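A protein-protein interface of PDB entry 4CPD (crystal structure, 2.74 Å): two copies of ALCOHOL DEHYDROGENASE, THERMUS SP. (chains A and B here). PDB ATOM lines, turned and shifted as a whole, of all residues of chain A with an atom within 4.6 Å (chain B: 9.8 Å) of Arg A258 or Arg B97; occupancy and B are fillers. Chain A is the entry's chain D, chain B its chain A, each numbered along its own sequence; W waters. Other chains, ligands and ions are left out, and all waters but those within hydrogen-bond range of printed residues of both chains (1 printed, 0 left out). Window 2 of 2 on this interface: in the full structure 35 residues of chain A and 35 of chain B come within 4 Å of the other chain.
The backbone NH of Tyr B94 sits close to the side-chain sulfur of Cys B92 (3.7 Å). OD1 of Asp A238 lies within salt-bridge range of NE of Arg A258, at 2.7 Å. The backbone carbonyl oxygen of Lys A284 sits at hydrogen-bond distance from the backbone NH of Gly A260 (2.8 Å). The guanidinium group (NH1) of Arg A258 sits at hydrogen-bond distance from the backbone carbonyl oxygen (O) of Gly A260 (3.4 Å). The side-chain amino group (NZ) of Lys A284 sits at hydrogen-bond distance from the backbone carbonyl oxygen (O) of Val A257, 2.8 Å away. O of Tyr B94 is in hydrogen-bond range of N of Gln B99.
Hydrophobic or aromatic side chains of chain B that line the printed part of chain A: Pro B93, Tyr B94 and Leu B102. Of the 12 printed residues of chain A, 5 touch a printed residue of chain B. Among the printed residues, Asp or Glu carboxylates within 4 Å of a Lys or Arg side-chain nitrogen of the other chain: Glu A235 with Arg B97 (2.8 Å).
Printed residues of chain B within 4 Å of Arg A258: Tyr B94, Arg B97 and Gln B99. Of chain A, only Glu A235 and Arg A258 come within 4 Å of Arg B97. Gly A236 touches none of the printed residues of chain B. No residue of chain B comes within 4 Å of Pro A237. No residue of chain B comes within 4 Å of Val A257. Of the printed residues of chain B, Pro A259 touches Tyr B94 and Leu B102. No residue of chain B comes within 4 Å of Gly A261. Of the printed residues of chain A, Leu B102 touches Pro A259, Gly A260 and Lys A284. Of the printed residues of chain A, Gln B99 touches Arg A258 (2.8 Å) and Gly A260 (2.9 Å). His B98 touches none of the printed residues of chain A. Arg B289 touches none of the printed residues of chain A. The nearest residue of chain B that does not touch Arg A258 is Leu B102 (5.0 Å). The nearest printed residue of chain B that does not touch Lys A284 is Ile B290 (5.2 Å).
Water W1 bridges NE of Arg B97 and OD1 of Asp A238.
O of Gly A260 is in hydrogen-bond range of NE2 of Gln B99 (2.9 Å). The guanidinium group (NH2) of Arg B97 lies within salt-bridge range of the side-chain carboxylate (OE1) of Glu A235 (2.8 Å). NE of Arg B97 lies close to NH2 of Arg A258. The side-chain amide oxygen (OE1) of Gln B99 is in hydrogen-bond range of the guanidinium group (NH1) of Arg A258, 2.8 Å away.
No position is printed for both chains.
Glu A235 touches Pro B93 (OE2 to CB, 3.8 Å). Glu A235 touches Tyr B94. Tyr B94 touches Arg A258 (CE1 to NH1, 3.7 Å). Pro A259 touches Tyr B94. Pro A259 touches Leu B102 (C to CD1, 3.6 Å). Gly A260 touches Leu B102 (N to CD1, 3.4 Å). O of Lys A284 touches CD2 of Leu B102, at 3.98 Å.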
ATOM      1  N   GLU A 235      24.522   7.171  26.728  1.00  0.00           N
ATOM      2  CA  GLU A 235      23.157   7.151  26.223  1.00  0.00           C
ATOM      3  C   GLU A 235      22.497   5.767  26.413  1.00  0.00           C
ATOM      4  O   GLU A 235      21.412   5.622  27.000  1.00  0.00           O
ATOM      5  CB  GLU A 235      23.177   7.512  24.745  1.00  0.00           C
ATOM      6  CG  GLU A 235      23.741   8.887  24.443  1.00  0.00           C
ATOM      7  CD  GLU A 235      23.787   9.187  22.952  1.00  0.00           C
ATOM      8  OE1 GLU A 235      23.845   8.245  22.103  1.00  0.00           O
ATOM      9  OE2 GLU A 235      23.767  10.387  22.625  1.00  0.00           O
ATOM     10  N   GLY A 236      23.205   4.758  25.927  1.00  0.00           N
ATOM     11  CA  GLY A 236      22.690   3.412  25.774  1.00  0.00           C
ATOM     12  C   GLY A 236      22.806   3.118  24.288  1.00  0.00           C
ATOM     13  O   GLY A 236      22.999   4.040  23.474  1.00  0.00           O
ATOM     14  N   PRO A 237      22.657   1.843  23.916  1.00  0.00           N
ATOM     15  CA  PRO A 237      22.681   1.436  22.522  1.00  0.00           C
ATOM     16  C   PRO A 237      21.384   1.781  21.758  1.00  0.00           C
ATOM     17  O   PRO A 237      20.275   1.874  22.361  1.00  0.00           O
ATOM     18  CB  PRO A 237      22.857  -0.077  22.616  1.00  0.00           C
ATOM     19  CG  PRO A 237      22.151  -0.441  23.852  1.00  0.00           C
ATOM     20  CD  PRO A 237      22.279   0.738  24.796  1.00  0.00           C
ATOM     21  N   ASP A 238      21.531   1.948  20.440  1.00  0.00           N
ATOM     22  CA  ASP A 238      20.398   2.212  19.564  1.00  0.00           C
ATOM     23  C   ASP A 238      19.365   1.082  19.596  1.00  0.00           C
ATOM     24  O   ASP A 238      18.139   1.324  19.552  1.00  0.00           O
ATOM     25  CB  ASP A 238      20.894   2.417  18.147  1.00  0.00           C
ATOM     26  CG  ASP A 238      21.841   3.563  18.041  1.00  0.00           C
ATOM     27  OD1 ASP A 238      21.361   4.710  18.168  1.00  0.00           O
ATOM     28  OD2 ASP A 238      23.049   3.324  17.862  1.00  0.00           O
ATOM     29  N   MET A 256      18.330  -0.346  29.650  1.00  0.00           N
ATOM     30  CA  MET A 256      19.583  -0.244  28.981  1.00  0.00           C
ATOM     31  C   MET A 256      19.497   0.631  27.727  1.00  0.00           C
ATOM     32  O   MET A 256      20.377   1.475  27.489  1.00  0.00           O
ATOM     33  CB  MET A 256      19.977  -1.681  28.671  1.00  0.00           C
ATOM     34  CG  MET A 256      21.284  -1.890  27.975  1.00  0.00           C
ATOM     35  SD  MET A 256      21.520  -3.666  27.739  1.00  0.00           S
ATOM     36  CE  MET A 256      21.594  -4.232  29.429  1.00  0.00           C
ATOM     37  N   VAL A 257      18.440   0.439  26.929  1.00  0.00           N
ATOM     38  CA  VAL A 257      18.349   1.062  25.597  1.00  0.00           C
ATOM     39  C   VAL A 257      18.325   2.571  25.708  1.00  0.00           C
ATOM     40  O   VAL A 257      17.798   3.116  26.649  1.00  0.00           O
ATOM     41  CB  VAL A 257      17.096   0.616  24.853  1.00  0.00           C
ATOM     42  CG1 VAL A 257      15.835   1.161  25.515  1.00  0.00           C
ATOM     43  CG2 VAL A 257      17.183   1.010  23.379  1.00  0.00           C
ATOM     44  N   ARG A 258      18.910   3.263  24.759  1.00  0.00           N
ATOM     45  CA  ARG A 258      18.887   4.708  24.823  1.00  0.00           C
ATOM     46  C   ARG A 258      17.491   5.216  24.628  1.00  0.00           C
ATOM     47  O   ARG A 258      16.667   4.532  24.011  1.00  0.00           O
ATOM     48  CB  ARG A 258      19.798   5.343  23.757  1.00  0.00           C
ATOM     49  CG  ARG A 258      19.340   5.233  22.303  1.00  0.00           C
ATOM     50  CD  ARG A 258      20.203   6.147  21.445  1.00  0.00           C
ATOM     51  NE  ARG A 258      19.926   6.033  20.012  1.00  0.00           N
ATOM     52  CZ  ARG A 258      18.879   6.574  19.365  1.00  0.00           C
ATOM     53  NH1 ARG A 258      17.919   7.282  19.981  1.00  0.00           N
ATOM     54  NH2 ARG A 258      18.791   6.365  18.077  1.00  0.00           N
ATOM     55  N   PRO A 259      17.226   6.441  25.113  1.00  0.00           N
ATOM     56  CA  PRO A 259      16.027   7.146  24.737  1.00  0.00           C
ATOM     57  C   PRO A 259      15.881   7.188  23.219  1.00  0.00           C
ATOM     58  O   PRO A 259      16.886   7.424  22.497  1.00  0.00           O
ATOM     59  CB  PRO A 259      16.287   8.549  25.259  1.00  0.00           C
ATOM     60  CG  PRO A 259      17.147   8.344  26.440  1.00  0.00           C
ATOM     61  CD  PRO A 259      18.052   7.240  26.033  1.00  0.00           C
ATOM     62  N   GLY A 260      14.654   6.925  22.747  1.00  0.00           N
ATOM     63  CA  GLY A 260      14.376   6.916  21.320  1.00  0.00           C
ATOM     64  C   GLY A 260      14.939   5.707  20.605  1.00  0.00           C
ATOM     65  O   GLY A 260      15.018   5.681  19.394  1.00  0.00           O
ATOM     66  N   GLY A 261      15.343   4.695  21.352  1.00  0.00           N
ATOM     67  CA  GLY A 261      15.848   3.486  20.741  1.00  0.00           C
ATOM     68  C   GLY A 261      14.753   2.429  20.636  1.00  0.00           C
ATOM     69  O   GLY A 261      13.549   2.687  20.854  1.00  0.00           O
ATOM     70  N   ARG A 262      15.191   1.211  20.353  1.00  0.00           N
ATOM     71  CA  ARG A 262      14.276   0.125  20.010  1.00  0.00           C
ATOM     72  C   ARG A 262      14.663  -1.137  20.686  1.00  0.00           C
ATOM     73  O   ARG A 262      15.828  -1.449  20.789  1.00  0.00           O
ATOM     74  CB  ARG A 262      14.367  -0.127  18.521  1.00  0.00           C
ATOM     75  CG  ARG A 262      13.876   1.026  17.654  1.00  0.00           C
ATOM     76  CD  ARG A 262      14.642   1.107  16.345  1.00  0.00           C
ATOM     77  NE  ARG A 262      15.734   2.081  16.413  1.00  0.00           N
ATOM     78  CZ  ARG A 262      17.016   1.870  16.105  1.00  0.00           C
ATOM     79  NH1 ARG A 262      17.468   0.702  15.672  1.00  0.00           N
ATOM     80  NH2 ARG A 262      17.869   2.877  16.223  1.00  0.00           N
ATOM     81  N   LYS A 284      11.162   8.574  27.793  1.00  0.00           N
ATOM     82  CA  LYS A 284      12.187   7.880  27.028  1.00  0.00           C
ATOM     83  C   LYS A 284      11.873   7.680  25.528  1.00  0.00           C
ATOM     84  O   LYS A 284      12.779   7.598  24.704  1.00  0.00           O
ATOM     85  CB  LYS A 284      12.479   6.532  27.690  1.00  0.00           C
ATOM     86  CG  LYS A 284      13.962   6.348  27.956  1.00  0.00           C
ATOM     87  CD  LYS A 284      14.252   4.960  28.503  1.00  0.00           C
ATOM     88  CE  LYS A 284      15.650   4.521  28.105  1.00  0.00           C
ATOM     89  NZ  LYS A 284      15.986   3.254  28.799  1.00  0.00           N
ATOM     90  N   CYS B  89      17.149  22.137  19.822  1.00  0.00           N
ATOM     91  CA  CYS B  89      18.322  22.939  19.602  1.00  0.00           C
ATOM     92  C   CYS B  89      18.841  22.773  18.190  1.00  0.00           C
ATOM     93  O   CYS B  89      19.494  23.666  17.667  1.00  0.00           O
ATOM     94  CB  CYS B  89      19.416  22.543  20.623  1.00  0.00           C
ATOM     95  SG  CYS B  89      20.342  21.018  20.236  1.00  0.00           S
ATOM     96  N   GLY B  90      18.651  21.586  17.626  1.00  0.00           N
ATOM     97  CA  GLY B  90      19.044  21.318  16.262  1.00  0.00           C
ATOM     98  C   GLY B  90      20.464  20.798  16.063  1.00  0.00           C
ATOM     99  O   GLY B  90      20.862  20.469  14.923  1.00  0.00           O
ATOM    100  N   THR B  91      21.251  20.737  17.135  1.00  0.00           N
ATOM    101  CA  THR B  91      22.661  20.311  16.997  1.00  0.00           C
ATOM    102  C   THR B  91      23.089  19.183  17.939  1.00  0.00           C
ATOM    103  O   THR B  91      24.090  18.530  17.682  1.00  0.00           O
ATOM    104  CB  THR B  91      23.665  21.512  17.092  1.00  0.00           C
ATOM    105  OG1 THR B  91      23.467  22.234  18.326  1.00  0.00           O
ATOM    106  CG2 THR B  91      23.499  22.466  15.893  1.00  0.00           C
ATOM    107  N   CYS B  92      22.346  18.917  19.007  1.00  0.00           N
ATOM    108  CA  CYS B  92      22.685  17.777  19.851  1.00  0.00           C
ATOM    109  C   CYS B  92      22.481  16.447  19.117  1.00  0.00           C
ATOM    110  O   CYS B  92      21.795  16.379  18.084  1.00  0.00           O
ATOM    111  CB  CYS B  92      21.873  17.802  21.119  1.00  0.00           C
ATOM    112  SG  CYS B  92      20.175  17.308  20.958  1.00  0.00           S
ATOM    113  N   PRO B  93      23.071  15.361  19.646  1.00  0.00           N
ATOM    114  CA  PRO B  93      22.958  14.071  18.955  1.00  0.00           C
ATOM    115  C   PRO B  93      21.522  13.605  18.676  1.00  0.00           C
ATOM    116  O   PRO B  93      21.269  13.037  17.598  1.00  0.00           O
ATOM    117  CB  PRO B  93      23.655  13.106  19.913  1.00  0.00           C
ATOM    118  CG  PRO B  93      24.546  13.959  20.751  1.00  0.00           C
ATOM    119  CD  PRO B  93      23.803  15.230  20.918  1.00  0.00           C
ATOM    120  N   TYR B  94      20.617  13.850  19.622  1.00  0.00           N
ATOM    121  CA  TYR B  94      19.194  13.547  19.387  1.00  0.00           C
ATOM    122  C   TYR B  94      18.548  14.381  18.246  1.00  0.00           C
ATOM    123  O   TYR B  94      17.809  13.842  17.435  1.00  0.00           O
ATOM    124  CB  TYR B  94      18.385  13.623  20.698  1.00  0.00           C
ATOM    125  CG  TYR B  94      18.781  12.493  21.609  1.00  0.00           C
ATOM    126  CD1 TYR B  94      18.326  11.198  21.374  1.00  0.00           C
ATOM    127  CD2 TYR B  94      19.706  12.689  22.656  1.00  0.00           C
ATOM    128  CE1 TYR B  94      18.729  10.144  22.183  1.00  0.00           C
ATOM    129  CE2 TYR B  94      20.112  11.639  23.470  1.00  0.00           C
ATOM    130  CZ  TYR B  94      19.625  10.368  23.237  1.00  0.00           C
ATOM    131  OH  TYR B  94      20.026   9.317  24.053  1.00  0.00           O
ATOM    132  N   CYS B  95      18.847  15.671  18.179  1.00  0.00           N
ATOM    133  CA  CYS B  95      18.336  16.505  17.113  1.00  0.00           C
ATOM    134  C   CYS B  95      18.892  16.026  15.805  1.00  0.00           C
ATOM    135  O   CYS B  95      18.171  16.007  14.837  1.00  0.00           O
ATOM    136  CB  CYS B  95      18.686  17.993  17.308  1.00  0.00           C
ATOM    137  SG  CYS B  95      17.692  18.815  18.566  1.00  0.00           S
ATOM    138  N   ARG B  96      20.154  15.614  15.775  1.00  0.00           N
ATOM    139  CA  ARG B  96      20.753  15.131  14.507  1.00  0.00           C
ATOM    140  C   ARG B  96      20.123  13.820  13.992  1.00  0.00           C
ATOM    141  O   ARG B  96      20.126  13.571  12.795  1.00  0.00           O
ATOM    142  CB  ARG B  96      22.261  14.985  14.611  1.00  0.00           C
ATOM    143  CG  ARG B  96      22.910  16.194  15.262  1.00  0.00           C
ATOM    144  CD  ARG B  96      24.153  16.669  14.537  1.00  0.00           C
ATOM    145  NE  ARG B  96      23.845  17.820  13.703  1.00  0.00           N
ATOM    146  CZ  ARG B  96      24.458  19.010  13.747  1.00  0.00           C
ATOM    147  NH1 ARG B  96      25.483  19.255  14.571  1.00  0.00           N
ATOM    148  NH2 ARG B  96      24.057  19.965  12.925  1.00  0.00           N
ATOM    149  N   ARG B  97      19.586  13.013  14.913  1.00  0.00           N
ATOM    150  CA  ARG B  97      18.815  11.811  14.603  1.00  0.00           C
ATOM    151  C   ARG B  97      17.363  12.129  14.273  1.00  0.00           C
ATOM    152  O   ARG B  97      16.563  11.222  14.093  1.00  0.00           O
ATOM    153  CB  ARG B  97      18.800  10.855  15.808  1.00  0.00           C
ATOM    154  CG  ARG B  97      20.124  10.224  16.216  1.00  0.00           C
ATOM    155  CD  ARG B  97      19.934   9.489  17.546  1.00  0.00           C
ATOM    156  NE  ARG B  97      21.175   8.871  18.027  1.00  0.00           N
ATOM    157  CZ  ARG B  97      21.778   9.140  19.191  1.00  0.00           C
ATOM    158  NH1 ARG B  97      21.260   9.988  20.063  1.00  0.00           N
ATOM    159  NH2 ARG B  97      22.903   8.527  19.504  1.00  0.00           N
ATOM    160  N   HIS B  98      17.024  13.409  14.222  1.00  0.00           N
ATOM    161  CA  HIS B  98      15.649  13.871  14.004  1.00  0.00           C
ATOM    162  C   HIS B  98      14.658  13.413  15.063  1.00  0.00           C
ATOM    163  O   HIS B  98      13.437  13.244  14.773  1.00  0.00           O
ATOM    164  CB  HIS B  98      15.173  13.518  12.595  1.00  0.00           C
ATOM    165  CG  HIS B  98      16.100  14.009  11.521  1.00  0.00           C
ATOM    166  ND1 HIS B  98      16.252  13.383  10.302  1.00  0.00           N
ATOM    167  CD2 HIS B  98      16.924  15.080  11.490  1.00  0.00           C
ATOM    168  CE1 HIS B  98      17.122  14.047   9.565  1.00  0.00           C
ATOM    169  NE2 HIS B  98      17.549  15.080  10.265  1.00  0.00           N
ATOM    170  N   GLN B  99      15.179  13.249  16.282  1.00  0.00           N
ATOM    171  CA  GLN B  99      14.344  12.958  17.434  1.00  0.00           C
ATOM    172  C   GLN B  99      14.332  14.192  18.350  1.00  0.00           C
ATOM    173  O   GLN B  99      14.900  14.208  19.452  1.00  0.00           O
ATOM    174  CB  GLN B  99      14.858  11.723  18.148  1.00  0.00           C
ATOM    175  CG  GLN B  99      14.901  10.487  17.263  1.00  0.00           C
ATOM    176  CD  GLN B  99      15.329   9.252  18.032  1.00  0.00           C
ATOM    177  OE1 GLN B  99      16.392   9.241  18.639  1.00  0.00           O
ATOM    178  NE2 GLN B  99      14.502   8.216  18.015  1.00  0.00           N
ATOM    179  N   TYR B 100      13.649  15.225  17.870  1.00  0.00           N
ATOM    180  CA  TYR B 100      13.703  16.560  18.477  1.00  0.00           C
ATOM    181  C   TYR B 100      13.019  16.564  19.818  1.00  0.00           C
ATOM    182  O   TYR B 100      13.320  17.408  20.656  1.00  0.00           O
ATOM    183  CB  TYR B 100      13.082  17.634  17.560  1.00  0.00           C
ATOM    184  CG  TYR B 100      13.633  17.627  16.135  1.00  0.00           C
ATOM    185  CD1 TYR B 100      14.760  18.375  15.787  1.00  0.00           C
ATOM    186  CD2 TYR B 100      13.039  16.841  15.126  1.00  0.00           C
ATOM    187  CE1 TYR B 100      15.274  18.359  14.499  1.00  0.00           C
ATOM    188  CE2 TYR B 100      13.550  16.828  13.837  1.00  0.00           C
ATOM    189  CZ  TYR B 100      14.662  17.599  13.528  1.00  0.00           C
ATOM    190  OH  TYR B 100      15.162  17.557  12.250  1.00  0.00           O
ATOM    191  N   ASN B 101      12.084  15.655  20.036  1.00  0.00           N
ATOM    192  CA  ASN B 101      11.492  15.518  21.364  1.00  0.00           C
ATOM    193  C   ASN B 101      12.469  14.993  22.430  1.00  0.00           C
ATOM    194  O   ASN B 101      12.154  15.029  23.585  1.00  0.00           O
ATOM    195  CB  ASN B 101      10.288  14.575  21.326  1.00  0.00           C
ATOM    196  CG  ASN B 101      10.625  13.211  20.765  1.00  0.00           C
ATOM    197  OD1 ASN B 101      11.296  13.102  19.739  1.00  0.00           O
ATOM    198  ND2 ASN B 101      10.212  12.172  21.456  1.00  0.00           N
ATOM    199  N   LEU B 102      13.628  14.463  22.034  1.00  0.00           N
ATOM    200  CA  LEU B 102      14.636  14.035  22.997  1.00  0.00           C
ATOM    201  C   LEU B 102      15.819  14.976  23.062  1.00  0.00           C
ATOM    202  O   LEU B 102      16.877  14.586  23.586  1.00  0.00           O
ATOM    203  CB  LEU B 102      15.120  12.640  22.623  1.00  0.00           C
ATOM    204  CG  LEU B 102      13.985  11.610  22.628  1.00  0.00           C
ATOM    205  CD1 LEU B 102      14.505  10.270  22.112  1.00  0.00           C
ATOM    206  CD2 LEU B 102      13.375  11.476  24.017  1.00  0.00           C
ATOM    207  N   CYS B 103      15.645  16.195  22.530  1.00  0.00           N
ATOM    208  CA  CYS B 103      16.713  17.205  22.488  1.00  0.00           C
ATOM    209  C   CYS B 103      17.298  17.372  23.877  1.00  0.00           C
ATOM    210  O   CYS B 103      16.563  17.428  24.859  1.00  0.00           O
ATOM    211  CB  CYS B 103      16.188  18.551  22.034  1.00  0.00           C
ATOM    212  SG  CYS B 103      17.467  19.806  22.089  1.00  0.00           S
ATOM    213  N   GLU B 104      18.621  17.424  23.946  1.00  0.00           N
ATOM    214  CA  GLU B 104      19.330  17.550  25.235  1.00  0.00           C
ATOM    215  C   GLU B 104      19.139  18.916  25.894  1.00  0.00           C
ATOM    216  O   GLU B 104      19.165  19.022  27.101  1.00  0.00           O
ATOM    217  CB  GLU B 104      20.820  17.217  25.079  1.00  0.00           C
ATOM    218  CG  GLU B 104      21.125  15.755  25.432  1.00  0.00           C
ATOM    219  CD  GLU B 104      22.352  15.226  24.728  1.00  0.00           C
ATOM    220  OE1 GLU B 104      23.037  16.066  24.100  1.00  0.00           O
ATOM    221  OE2 GLU B 104      22.622  13.992  24.784  1.00  0.00           O
ATOM    222  N   ARG B 289       4.612   1.318  21.029  1.00  0.00           N
ATOM    223  CA  ARG B 289       5.409   2.513  21.159  1.00  0.00           C
ATOM    224  C   ARG B 289       4.721   3.503  22.104  1.00  0.00           C
ATOM    225  O   ARG B 289       3.517   3.681  22.070  1.00  0.00           O
ATOM    226  CB  ARG B 289       5.721   3.130  19.797  1.00  0.00           C
ATOM    227  CG  ARG B 289       6.714   4.283  19.936  1.00  0.00           C
ATOM    228  CD  ARG B 289       7.199   4.823  18.605  1.00  0.00           C
ATOM    229  NE  ARG B 289       8.161   5.907  18.780  1.00  0.00           N
ATOM    230  CZ  ARG B 289       8.780   6.544  17.786  1.00  0.00           C
ATOM    231  NH1 ARG B 289       8.563   6.223  16.519  1.00  0.00           N
ATOM    232  NH2 ARG B 289       9.627   7.515  18.059  1.00  0.00           N
ATOM    233  N   ILE B 290       5.516   4.137  22.951  1.00  0.00           N
ATOM    234  CA  ILE B 290       5.019   5.133  23.901  1.00  0.00           C
ATOM    235  C   ILE B 290       5.996   6.290  23.956  1.00  0.00           C
ATOM    236  O   ILE B 290       7.198   6.083  23.978  1.00  0.00           O
ATOM    237  CB  ILE B 290       4.802   4.536  25.309  1.00  0.00           C
ATOM    238  CG1 ILE B 290       4.327   5.613  26.287  1.00  0.00           C
ATOM    239  CG2 ILE B 290       6.061   3.861  25.849  1.00  0.00           C
ATOM    240  CD1 ILE B 290       3.553   5.042  27.460  1.00  0.00           C
ATOM    241  N   ASN B 294       6.879  14.172  18.618  1.00  0.00           N
ATOM    242  CA  ASN B 294       8.081  14.706  17.966  1.00  0.00           C
ATOM    243  C   ASN B 294       7.579  15.604  16.844  1.00  0.00           C
ATOM    244  O   ASN B 294       7.771  15.373  15.641  1.00  0.00           O
ATOM    245  CB  ASN B 294       8.949  13.571  17.448  1.00  0.00           C
ATOM    246  CG  ASN B 294      10.191  14.056  16.747  1.00  0.00           C
ATOM    247  OD1 ASN B 294      10.648  15.171  16.964  1.00  0.00           O
ATOM    248  ND2 ASN B 294      10.750  13.224  15.901  1.00  0.00           N
ATOM    249  N   LEU B 297       9.086  16.716  13.370  1.00  0.00           N
ATOM    250  CA  LEU B 297       9.220  15.766  12.306  1.00  0.00           C
ATOM    251  C   LEU B 297       8.022  15.853  11.347  1.00  0.00           C
ATOM    252  O   LEU B 297       8.193  15.626  10.177  1.00  0.00           O
ATOM    253  CB  LEU B 297       9.356  14.346  12.878  1.00  0.00           C
ATOM    254  CG  LEU B 297       9.842  13.286  11.858  1.00  0.00           C
ATOM    255  CD1 LEU B 297      11.227  13.615  11.373  1.00  0.00           C
ATOM    256  CD2 LEU B 297       9.821  11.885  12.460  1.00  0.00           C
HETATM  257  O   HOH W   1      22.681   6.869  16.176  1.00  0.00           O
